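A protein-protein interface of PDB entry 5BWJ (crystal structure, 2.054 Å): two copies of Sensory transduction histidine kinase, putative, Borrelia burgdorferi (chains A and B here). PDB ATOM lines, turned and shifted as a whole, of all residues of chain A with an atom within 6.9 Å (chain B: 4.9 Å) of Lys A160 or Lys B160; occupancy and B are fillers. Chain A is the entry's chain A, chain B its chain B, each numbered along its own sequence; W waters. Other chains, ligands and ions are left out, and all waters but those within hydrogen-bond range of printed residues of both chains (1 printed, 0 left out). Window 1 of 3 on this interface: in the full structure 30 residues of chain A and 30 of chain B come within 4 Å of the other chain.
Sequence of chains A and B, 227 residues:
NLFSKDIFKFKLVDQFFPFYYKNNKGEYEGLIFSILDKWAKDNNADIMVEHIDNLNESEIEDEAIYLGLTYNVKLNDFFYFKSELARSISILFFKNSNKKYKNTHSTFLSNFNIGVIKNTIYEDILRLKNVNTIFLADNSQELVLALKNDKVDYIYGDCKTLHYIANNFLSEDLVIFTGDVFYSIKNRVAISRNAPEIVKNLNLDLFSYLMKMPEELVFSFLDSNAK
Phe A17 touches Cys B159, and with the chains exchanged Cys A159 touches Phe B17. Cys A159 touches Lys B160, but with the chains exchanged Lys A160 does not touch Cys B159 (5.0 Å). Lys A160 touches Phe B17, but with the chains exchanged Phe A17 does not touch Lys B160 (4.5 Å). Lys A160 touches its own counterpart, Lys B160. Positions printed for both chains: 17, 158, 159, 160, 161, 162, 163 and 164.
OG1 of Thr A161 lies within hydrogen-bond range of N of Phe A17, 3.2 Å away. OD1 of Asp B158 is in hydrogen-bond range of N of Lys B160. N of Lys A160 sits at hydrogen-bond distance from OD1 of Asp A158 (3.2 Å). N of Phe B17 lies within hydrogen-bond range of OG1 of Thr B161, at 3.1 Å. O of Ile A89 lies within hydrogen-bond range of N of Cys A159, 3.2 Å away.
Hydrophobic or aromatic side chains of chain B that line the printed part of chain A: Phe B17, His B163 and Tyr B164. Hydrophobic or aromatic side chains of chain A that line the printed part of chain B: Phe A17, His A163 and Tyr A164. Among the printed residues, 11 pairs touch across the chains.
O of Cys B159 touches CE2 of Phe A17 (3.7 Å). His B163 touches Phe A17. NZ of Lys B160 touches O of Arg A87 (3.8 Å). O of Cys A159 touches CZ of Phe B17, 3.8 Å away. SG of Cys A159 touches NZ of Lys B160 (3.8 Å). CE2 of Phe B17 touches CA of Lys A160, at 3.8 Å. Lys A160 touches His B163 (NZ to CD2, 3.5 Å). CE1 of Tyr B164 touches NE2 of His A163, at 3.3 Å. Tyr A164 touches His B163.
Of the printed residues of chain B, Arg A87 touches Lys B160 (3.8 Å). Of the printed residues of chain B, Cys A159 touches Phe B17 (3.8 Å) and Lys B160 (3.8 Å). Lys A160 touches just these residues of chain B: Phe B17 (3.8 Å), Lys B160 (3.1 Å), His B163 (3.5 Å) and Tyr B164 (3.4 Å). Asp B158 touches none of the printed residues of chain A. Of the printed residues of chain A, Cys B159 touches Phe A17 (3.7 Å). Lys B160 touches just these residues of chain A: Arg A87 (3.8 Å), Cys A159 (3.8 Å) and Lys A160 (3.1 Å). Printed residues of chain A within 4 Å of His B163: Phe A17 (3.8 Å), Lys A160 (3.5 Å) and Tyr A164 (3.3 Å). The nearest printed residue of chain B that does not touch Lys A160 is Cys B159 (5.0 Å). The nearest residue of chain A that does not touch Lys B160 is Phe A17 (4.5 Å).
Water W1 lies within hydrogen-bond range of O of Arg A87 (2.5 Å), OG of Ser A88 (3.0 Å) and NZ of Lys B160 (3.0 Å).
NZ of Lys A160 sits close to N of Tyr B164 (3.4 Å). O of Lys B160 sits at hydrogen-bond distance from NZ of Lys A160 (3.1 Å).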
ATOM      1  N   PHE A  17      22.735  11.124 -33.169  1.00  0.00           N
ATOM      2  CA  PHE A  17      21.565  10.272 -32.975  1.00  0.00           C
ATOM      3  C   PHE A  17      20.295  11.116 -33.056  1.00  0.00           C
ATOM      4  O   PHE A  17      20.254  12.214 -32.507  1.00  0.00           O
ATOM      5  CB  PHE A  17      21.646   9.552 -31.625  1.00  0.00           C
ATOM      6  CG  PHE A  17      20.477   8.647 -31.345  1.00  0.00           C
ATOM      7  CD1 PHE A  17      20.539   7.301 -31.659  1.00  0.00           C
ATOM      8  CD2 PHE A  17      19.320   9.143 -30.767  1.00  0.00           C
ATOM      9  CE1 PHE A  17      19.467   6.463 -31.401  1.00  0.00           C
ATOM     10  CE2 PHE A  17      18.245   8.311 -30.509  1.00  0.00           C
ATOM     11  CZ  PHE A  17      18.320   6.971 -30.827  1.00  0.00           C
ATOM     12  N   PRO A  18      19.246  10.613 -33.733  1.00  0.00           N
ATOM     13  CA  PRO A  18      19.112   9.324 -34.420  1.00  0.00           C
ATOM     14  C   PRO A  18      19.440   9.394 -35.912  1.00  0.00           C
ATOM     15  O   PRO A  18      19.272   8.401 -36.616  1.00  0.00           O
ATOM     16  CB  PRO A  18      17.638   8.994 -34.215  1.00  0.00           C
ATOM     17  CG  PRO A  18      16.972  10.341 -34.285  1.00  0.00           C
ATOM     18  CD  PRO A  18      17.968  11.348 -33.737  1.00  0.00           C
ATOM     19  N   ALA A  86      16.995  18.461 -35.596  1.00  0.00           N
ATOM     20  CA  ALA A  86      16.578  18.337 -34.204  1.00  0.00           C
ATOM     21  C   ALA A  86      17.459  19.200 -33.304  1.00  0.00           C
ATOM     22  O   ALA A  86      18.627  19.430 -33.607  1.00  0.00           O
ATOM     23  CB  ALA A  86      16.626  16.882 -33.762  1.00  0.00           C
ATOM     24  N   ARG A  87      16.890  19.688 -32.206  1.00  0.00           N
ATOM     25  CA  ARG A  87      17.651  20.444 -31.218  1.00  0.00           C
ATOM     26  C   ARG A  87      18.285  19.498 -30.203  1.00  0.00           C
ATOM     27  O   ARG A  87      17.843  18.361 -30.042  1.00  0.00           O
ATOM     28  CB  ARG A  87      16.760  21.456 -30.495  1.00  0.00           C
ATOM     29  CG  ARG A  87      16.259  22.597 -31.365  1.00  0.00           C
ATOM     30  CD  ARG A  87      15.809  23.774 -30.511  1.00  0.00           C
ATOM     31  NE  ARG A  87      15.312  24.889 -31.317  1.00  0.00           N
ATOM     32  CZ  ARG A  87      14.033  25.097 -31.622  1.00  0.00           C
ATOM     33  NH1 ARG A  87      13.087  24.270 -31.192  1.00  0.00           N
ATOM     34  NH2 ARG A  87      13.696  26.144 -32.363  1.00  0.00           N
ATOM     35  N   SER A  88      19.323  19.979 -29.524  1.00  0.00           N
ATOM     36  CA  SER A  88      19.991  19.215 -28.478  1.00  0.00           C
ATOM     37  C   SER A  88      20.128  20.063 -27.225  1.00  0.00           C
ATOM     38  O   SER A  88      19.843  21.262 -27.239  1.00  0.00           O
ATOM     39  CB  SER A  88      21.371  18.743 -28.944  1.00  0.00           C
ATOM     40  OG  SER A  88      21.266  17.829 -30.022  1.00  0.00           O
ATOM     41  N   ILE A  89      20.562  19.427 -26.143  1.00  0.00           N
ATOM     42  CA  ILE A  89      20.868  20.125 -24.903  1.00  0.00           C
ATOM     43  C   ILE A  89      22.293  19.785 -24.490  1.00  0.00           C
ATOM     44  O   ILE A  89      22.688  18.621 -24.485  1.00  0.00           O
ATOM     45  CB  ILE A  89      19.876  19.754 -23.784  1.00  0.00           C
ATOM     46  CG1 ILE A  89      18.462  20.186 -24.184  1.00  0.00           C
ATOM     47  CG2 ILE A  89      20.282  20.412 -22.463  1.00  0.00           C
ATOM     48  CD1 ILE A  89      17.373  19.741 -23.222  1.00  0.00           C
ATOM     49  N   ILE A  91      25.221  18.989 -22.102  1.00  0.00           N
ATOM     50  CA  ILE A  91      25.340  18.354 -20.795  1.00  0.00           C
ATOM     51  C   ILE A  91      26.801  18.074 -20.472  1.00  0.00           C
ATOM     52  O   ILE A  91      27.583  17.690 -21.342  1.00  0.00           O
ATOM     53  CB  ILE A  91      24.533  17.037 -20.726  1.00  0.00           C
ATOM     54  CG1 ILE A  91      23.042  17.330 -20.925  1.00  0.00           C
ATOM     55  CG2 ILE A  91      24.762  16.326 -19.384  1.00  0.00           C
ATOM     56  CD1 ILE A  91      22.155  16.104 -20.923  1.00  0.00           C
ATOM     57  N   PHE A  93      29.057  15.588 -18.447  1.00  0.00           N
ATOM     58  CA  PHE A  93      29.028  14.248 -17.861  1.00  0.00           C
ATOM     59  C   PHE A  93      30.321  13.922 -17.122  1.00  0.00           C
ATOM     60  O   PHE A  93      31.388  14.411 -17.487  1.00  0.00           O
ATOM     61  CB  PHE A  93      28.810  13.183 -18.941  1.00  0.00           C
ATOM     62  CG  PHE A  93      27.457  13.226 -19.592  1.00  0.00           C
ATOM     63  CD1 PHE A  93      26.330  12.785 -18.917  1.00  0.00           C
ATOM     64  CD2 PHE A  93      27.318  13.668 -20.896  1.00  0.00           C
ATOM     65  CE1 PHE A  93      25.088  12.808 -19.521  1.00  0.00           C
ATOM     66  CE2 PHE A  93      26.077  13.694 -21.507  1.00  0.00           C
ATOM     67  CZ  PHE A  93      24.963  13.263 -20.821  1.00  0.00           C
ATOM     68  N   GLY A 157      29.048  18.011 -24.101  1.00  0.00           N
ATOM     69  CA  GLY A 157      28.536  17.898 -25.455  1.00  0.00           C
ATOM     70  C   GLY A 157      27.077  17.499 -25.565  1.00  0.00           C
ATOM     71  O   GLY A 157      26.274  17.744 -24.665  1.00  0.00           O
ATOM     72  N   ASP A 158      26.747  16.876 -26.693  1.00  0.00           N
ATOM     73  CA  ASP A 158      25.383  16.473 -27.008  1.00  0.00           C
ATOM     74  C   ASP A 158      24.814  15.517 -25.960  1.00  0.00           C
ATOM     75  O   ASP A 158      25.471  14.550 -25.576  1.00  0.00           O
ATOM     76  CB  ASP A 158      25.348  15.814 -28.386  1.00  0.00           C
ATOM     77  CG  ASP A 158      23.945  15.491 -28.841  1.00  0.00           C
ATOM     78  OD1 ASP A 158      23.490  14.354 -28.600  1.00  0.00           O
ATOM     79  OD2 ASP A 158      23.296  16.373 -29.442  1.00  0.00           O
ATOM     80  N   CYS A 159      23.587  15.783 -25.516  1.00  0.00           N
ATOM     81  CA  CYS A 159      22.956  14.995 -24.458  1.00  0.00           C
ATOM     82  C   CYS A 159      22.870  13.505 -24.799  1.00  0.00           C
ATOM     83  O   CYS A 159      23.377  12.668 -24.055  1.00  0.00           O
ATOM     84  CB  CYS A 159      21.552  15.540 -24.139  1.00  0.00           C
ATOM     85  SG  CYS A 159      20.417  15.764 -25.553  1.00  0.00           S
ATOM     86  N   LYS A 160      22.244  13.173 -25.924  1.00  0.00           N
ATOM     87  CA  LYS A 160      21.977  11.775 -26.254  1.00  0.00           C
ATOM     88  C   LYS A 160      23.175  11.067 -26.885  1.00  0.00           C
ATOM     89  O   LYS A 160      23.502   9.941 -26.507  1.00  0.00           O
ATOM     90  CB  LYS A 160      20.772  11.680 -27.192  1.00  0.00           C
ATOM     91  CG  LYS A 160      20.422  10.262 -27.644  1.00  0.00           C
ATOM     92  CD  LYS A 160      20.062   9.355 -26.474  1.00  0.00           C
ATOM     93  CE  LYS A 160      19.689   7.955 -26.952  1.00  0.00           C
ATOM     94  NZ  LYS A 160      19.199   7.086 -25.845  1.00  0.00           N
ATOM     95  N   THR A 161      23.823  11.719 -27.845  1.00  0.00           N
ATOM     96  CA  THR A 161      24.886  11.080 -28.615  1.00  0.00           C
ATOM     97  C   THR A 161      26.072  10.689 -27.738  1.00  0.00           C
ATOM     98  O   THR A 161      26.579   9.570 -27.844  1.00  0.00           O
ATOM     99  CB  THR A 161      25.374  11.992 -29.763  1.00  0.00           C
ATOM    100  OG1 THR A 161      24.285  12.246 -30.660  1.00  0.00           O
ATOM    101  CG2 THR A 161      26.509  11.340 -30.546  1.00  0.00           C
ATOM    102  N   LEU A 162      26.518  11.593 -26.871  1.00  0.00           N
ATOM    103  CA  LEU A 162      27.641  11.282 -25.989  1.00  0.00           C
ATOM    104  C   LEU A 162      27.266  10.220 -24.969  1.00  0.00           C
ATOM    105  O   LEU A 162      28.068   9.335 -24.665  1.00  0.00           O
ATOM    106  CB  LEU A 162      28.139  12.529 -25.258  1.00  0.00           C
ATOM    107  CG  LEU A 162      29.048  13.489 -26.026  1.00  0.00           C
ATOM    108  CD1 LEU A 162      29.515  14.594 -25.092  1.00  0.00           C
ATOM    109  CD2 LEU A 162      30.245  12.775 -26.644  1.00  0.00           C
ATOM    110  N   HIS A 163      26.056  10.310 -24.432  1.00  0.00           N
ATOM    111  CA  HIS A 163      25.600   9.335 -23.453  1.00  0.00           C
ATOM    112  C   HIS A 163      25.565   7.958 -24.097  1.00  0.00           C
ATOM    113  O   HIS A 163      25.984   6.968 -23.503  1.00  0.00           O
ATOM    114  CB  HIS A 163      24.219   9.706 -22.909  1.00  0.00           C
ATOM    115  CG  HIS A 163      23.751   8.815 -21.802  1.00  0.00           C
ATOM    116  ND1 HIS A 163      23.804   9.184 -20.476  1.00  0.00           N
ATOM    117  CD2 HIS A 163      23.230   7.565 -21.824  1.00  0.00           C
ATOM    118  CE1 HIS A 163      23.331   8.204 -19.727  1.00  0.00           C
ATOM    119  NE2 HIS A 163      22.977   7.209 -20.521  1.00  0.00           N
ATOM    120  N   TYR A 164      25.078   7.913 -25.330  1.00  0.00           N
ATOM    121  CA  TYR A 164      24.971   6.664 -26.073  1.00  0.00           C
ATOM    122  C   TYR A 164      26.333   6.021 -26.330  1.00  0.00           C
ATOM    123  O   TYR A 164      26.543   4.851 -26.014  1.00  0.00           O
ATOM    124  CB  TYR A 164      24.258   6.910 -27.398  1.00  0.00           C
ATOM    125  CG  TYR A 164      24.192   5.688 -28.273  1.00  0.00           C
ATOM    126  CD1 TYR A 164      23.391   4.610 -27.927  1.00  0.00           C
ATOM    127  CD2 TYR A 164      24.931   5.609 -29.446  1.00  0.00           C
ATOM    128  CE1 TYR A 164      23.330   3.491 -28.719  1.00  0.00           C
ATOM    129  CE2 TYR A 164      24.872   4.491 -30.247  1.00  0.00           C
ATOM    130  CZ  TYR A 164      24.067   3.436 -29.877  1.00  0.00           C
ATOM    131  OH  TYR A 164      23.994   2.317 -30.665  1.00  0.00           O
ATOM    132  N   ILE A 165      27.254   6.783 -26.908  1.00  0.00           N
ATOM    133  CA  ILE A 165      28.584   6.267 -27.208  1.00  0.00           C
ATOM    134  C   ILE A 165      29.306   5.877 -25.917  1.00  0.00           C
ATOM    135  O   ILE A 165      30.032   4.885 -25.878  1.00  0.00           O
ATOM    136  CB  ILE A 165      29.414   7.298 -28.001  1.00  0.00           C
ATOM    137  CG1 ILE A 165      28.762   7.537 -29.365  1.00  0.00           C
ATOM    138  CG2 ILE A 165      30.853   6.819 -28.198  1.00  0.00           C
ATOM    139  CD1 ILE A 165      29.307   8.733 -30.116  1.00  0.00           C
ATOM    140  N   ALA A 166      29.086   6.648 -24.857  1.00  0.00           N
ATOM    141  CA  ALA A 166      29.696   6.362 -23.563  1.00  0.00           C
ATOM    142  C   ALA A 166      29.279   4.987 -23.049  1.00  0.00           C
ATOM    143  O   ALA A 166      30.111   4.215 -22.565  1.00  0.00           O
ATOM    144  CB  ALA A 166      29.326   7.437 -22.554  1.00  0.00           C
ATOM    145  N   PHE B  17      14.050  11.603 -21.292  1.00  0.00           N
ATOM    146  CA  PHE B  17      15.477  11.874 -21.431  1.00  0.00           C
ATOM    147  C   PHE B  17      15.691  13.153 -22.235  1.00  0.00           C
ATOM    148  O   PHE B  17      15.041  13.345 -23.261  1.00  0.00           O
ATOM    149  CB  PHE B  17      16.185  10.699 -22.111  1.00  0.00           C
ATOM    150  CG  PHE B  17      17.685  10.836 -22.161  1.00  0.00           C
ATOM    151  CD1 PHE B  17      18.478  10.214 -21.210  1.00  0.00           C
ATOM    152  CD2 PHE B  17      18.301  11.583 -23.154  1.00  0.00           C
ATOM    153  CE1 PHE B  17      19.856  10.335 -21.247  1.00  0.00           C
ATOM    154  CE2 PHE B  17      19.678  11.709 -23.196  1.00  0.00           C
ATOM    155  CZ  PHE B  17      20.457  11.082 -22.241  1.00  0.00           C
ATOM    156  N   ASP B 158       8.918   7.810 -28.059  1.00  0.00           N
ATOM    157  CA  ASP B 158       9.999   8.787 -27.983  1.00  0.00           C
ATOM    158  C   ASP B 158      11.343   8.200 -28.410  1.00  0.00           C
ATOM    159  O   ASP B 158      11.752   7.148 -27.919  1.00  0.00           O
ATOM    160  CB  ASP B 158      10.099   9.335 -26.558  1.00  0.00           C
ATOM    161  CG  ASP B 158      11.105  10.458 -26.437  1.00  0.00           C
ATOM    162  OD1 ASP B 158      12.286  10.169 -26.158  1.00  0.00           O
ATOM    163  OD2 ASP B 158      10.714  11.630 -26.623  1.00  0.00           O
ATOM    164  N   CYS B 159      12.028   8.901 -29.310  1.00  0.00           N
ATOM    165  CA  CYS B 159      13.275   8.405 -29.894  1.00  0.00           C
ATOM    166  C   CYS B 159      14.385   8.241 -28.862  1.00  0.00           C
ATOM    167  O   CYS B 159      15.129   7.261 -28.898  1.00  0.00           O
ATOM    168  CB  CYS B 159      13.759   9.341 -31.009  1.00  0.00           C
ATOM    169  SG  CYS B 159      14.102  11.047 -30.489  1.00  0.00           S
ATOM    170  N   LYS B 160      14.499   9.201 -27.950  1.00  0.00           N
ATOM    171  CA  LYS B 160      15.589   9.194 -26.978  1.00  0.00           C
ATOM    172  C   LYS B 160      15.285   8.328 -25.757  1.00  0.00           C
ATOM    173  O   LYS B 160      16.143   7.574 -25.300  1.00  0.00           O
ATOM    174  CB  LYS B 160      15.904  10.626 -26.531  1.00  0.00           C
ATOM    175  CG  LYS B 160      16.569  11.471 -27.608  1.00  0.00           C
ATOM    176  CD  LYS B 160      16.778  12.908 -27.157  1.00  0.00           C
ATOM    177  CE  LYS B 160      17.376  13.752 -28.275  1.00  0.00           C
ATOM    178  NZ  LYS B 160      17.449  15.194 -27.913  1.00  0.00           N
ATOM    179  N   THR B 161      14.065   8.425 -25.237  1.00  0.00           N
ATOM    180  CA  THR B 161      13.732   7.794 -23.959  1.00  0.00           C
ATOM    181  C   THR B 161      13.600   6.276 -24.062  1.00  0.00           C
ATOM    182  O   THR B 161      14.167   5.544 -23.247  1.00  0.00           O
ATOM    183  CB  THR B 161      12.420   8.359 -23.379  1.00  0.00           C
ATOM    184  OG1 THR B 161      12.529   9.780 -23.246  1.00  0.00           O
ATOM    185  CG2 THR B 161      12.127   7.750 -22.006  1.00  0.00           C
ATOM    186  N   LEU B 162      12.841   5.803 -25.044  1.00  0.00           N
ATOM    187  CA  LEU B 162      12.640   4.367 -25.204  1.00  0.00           C
ATOM    188  C   LEU B 162      13.963   3.686 -25.513  1.00  0.00           C
ATOM    189  O   LEU B 162      14.239   2.582 -25.036  1.00  0.00           O
ATOM    190  CB  LEU B 162      11.625   4.080 -26.310  1.00  0.00           C
ATOM    191  CG  LEU B 162      10.208   4.607 -26.079  1.00  0.00           C
ATOM    192  CD1 LEU B 162       9.302   4.157 -27.209  1.00  0.00           C
ATOM    193  CD2 LEU B 162       9.652   4.153 -24.731  1.00  0.00           C
ATOM    194  N   HIS B 163      14.785   4.364 -26.305  1.00  0.00           N
ATOM    195  CA  HIS B 163      16.086   3.843 -26.678  1.00  0.00           C
ATOM    196  C   HIS B 163      17.025   3.795 -25.478  1.00  0.00           C
ATOM    197  O   HIS B 163      17.771   2.831 -25.303  1.00  0.00           O
ATOM    198  CB  HIS B 163      16.700   4.695 -27.784  1.00  0.00           C
ATOM    199  CG  HIS B 163      17.972   4.133 -28.330  1.00  0.00           C
ATOM    200  ND1 HIS B 163      17.998   3.263 -29.398  1.00  0.00           N
ATOM    201  CD2 HIS B 163      19.257   4.297 -27.944  1.00  0.00           C
ATOM    202  CE1 HIS B 163      19.248   2.923 -29.654  1.00  0.00           C
ATOM    203  NE2 HIS B 163      20.031   3.536 -28.784  1.00  0.00           N
ATOM    204  N   TYR B 164      16.990   4.842 -24.659  1.00  0.00           N
ATOM    205  CA  TYR B 164      17.826   4.899 -23.469  1.00  0.00           C
ATOM    206  C   TYR B 164      17.529   3.739 -22.523  1.00  0.00           C
ATOM    207  O   TYR B 164      18.441   3.041 -22.081  1.00  0.00           O
ATOM    208  CB  TYR B 164      17.630   6.221 -22.723  1.00  0.00           C
ATOM    209  CG  TYR B 164      18.124   6.158 -21.294  1.00  0.00           C
ATOM    210  CD1 TYR B 164      19.476   6.277 -21.001  1.00  0.00           C
ATOM    211  CD2 TYR B 164      17.241   5.958 -20.240  1.00  0.00           C
ATOM    212  CE1 TYR B 164      19.937   6.206 -19.697  1.00  0.00           C
ATOM    213  CE2 TYR B 164      17.693   5.888 -18.932  1.00  0.00           C
ATOM    214  CZ  TYR B 164      19.041   6.012 -18.668  1.00  0.00           C
ATOM    215  OH  TYR B 164      19.497   5.946 -17.370  1.00  0.00           O
HETATM  216  O   HOH W   1      18.892  16.095 -30.387  1.00  0.00           O
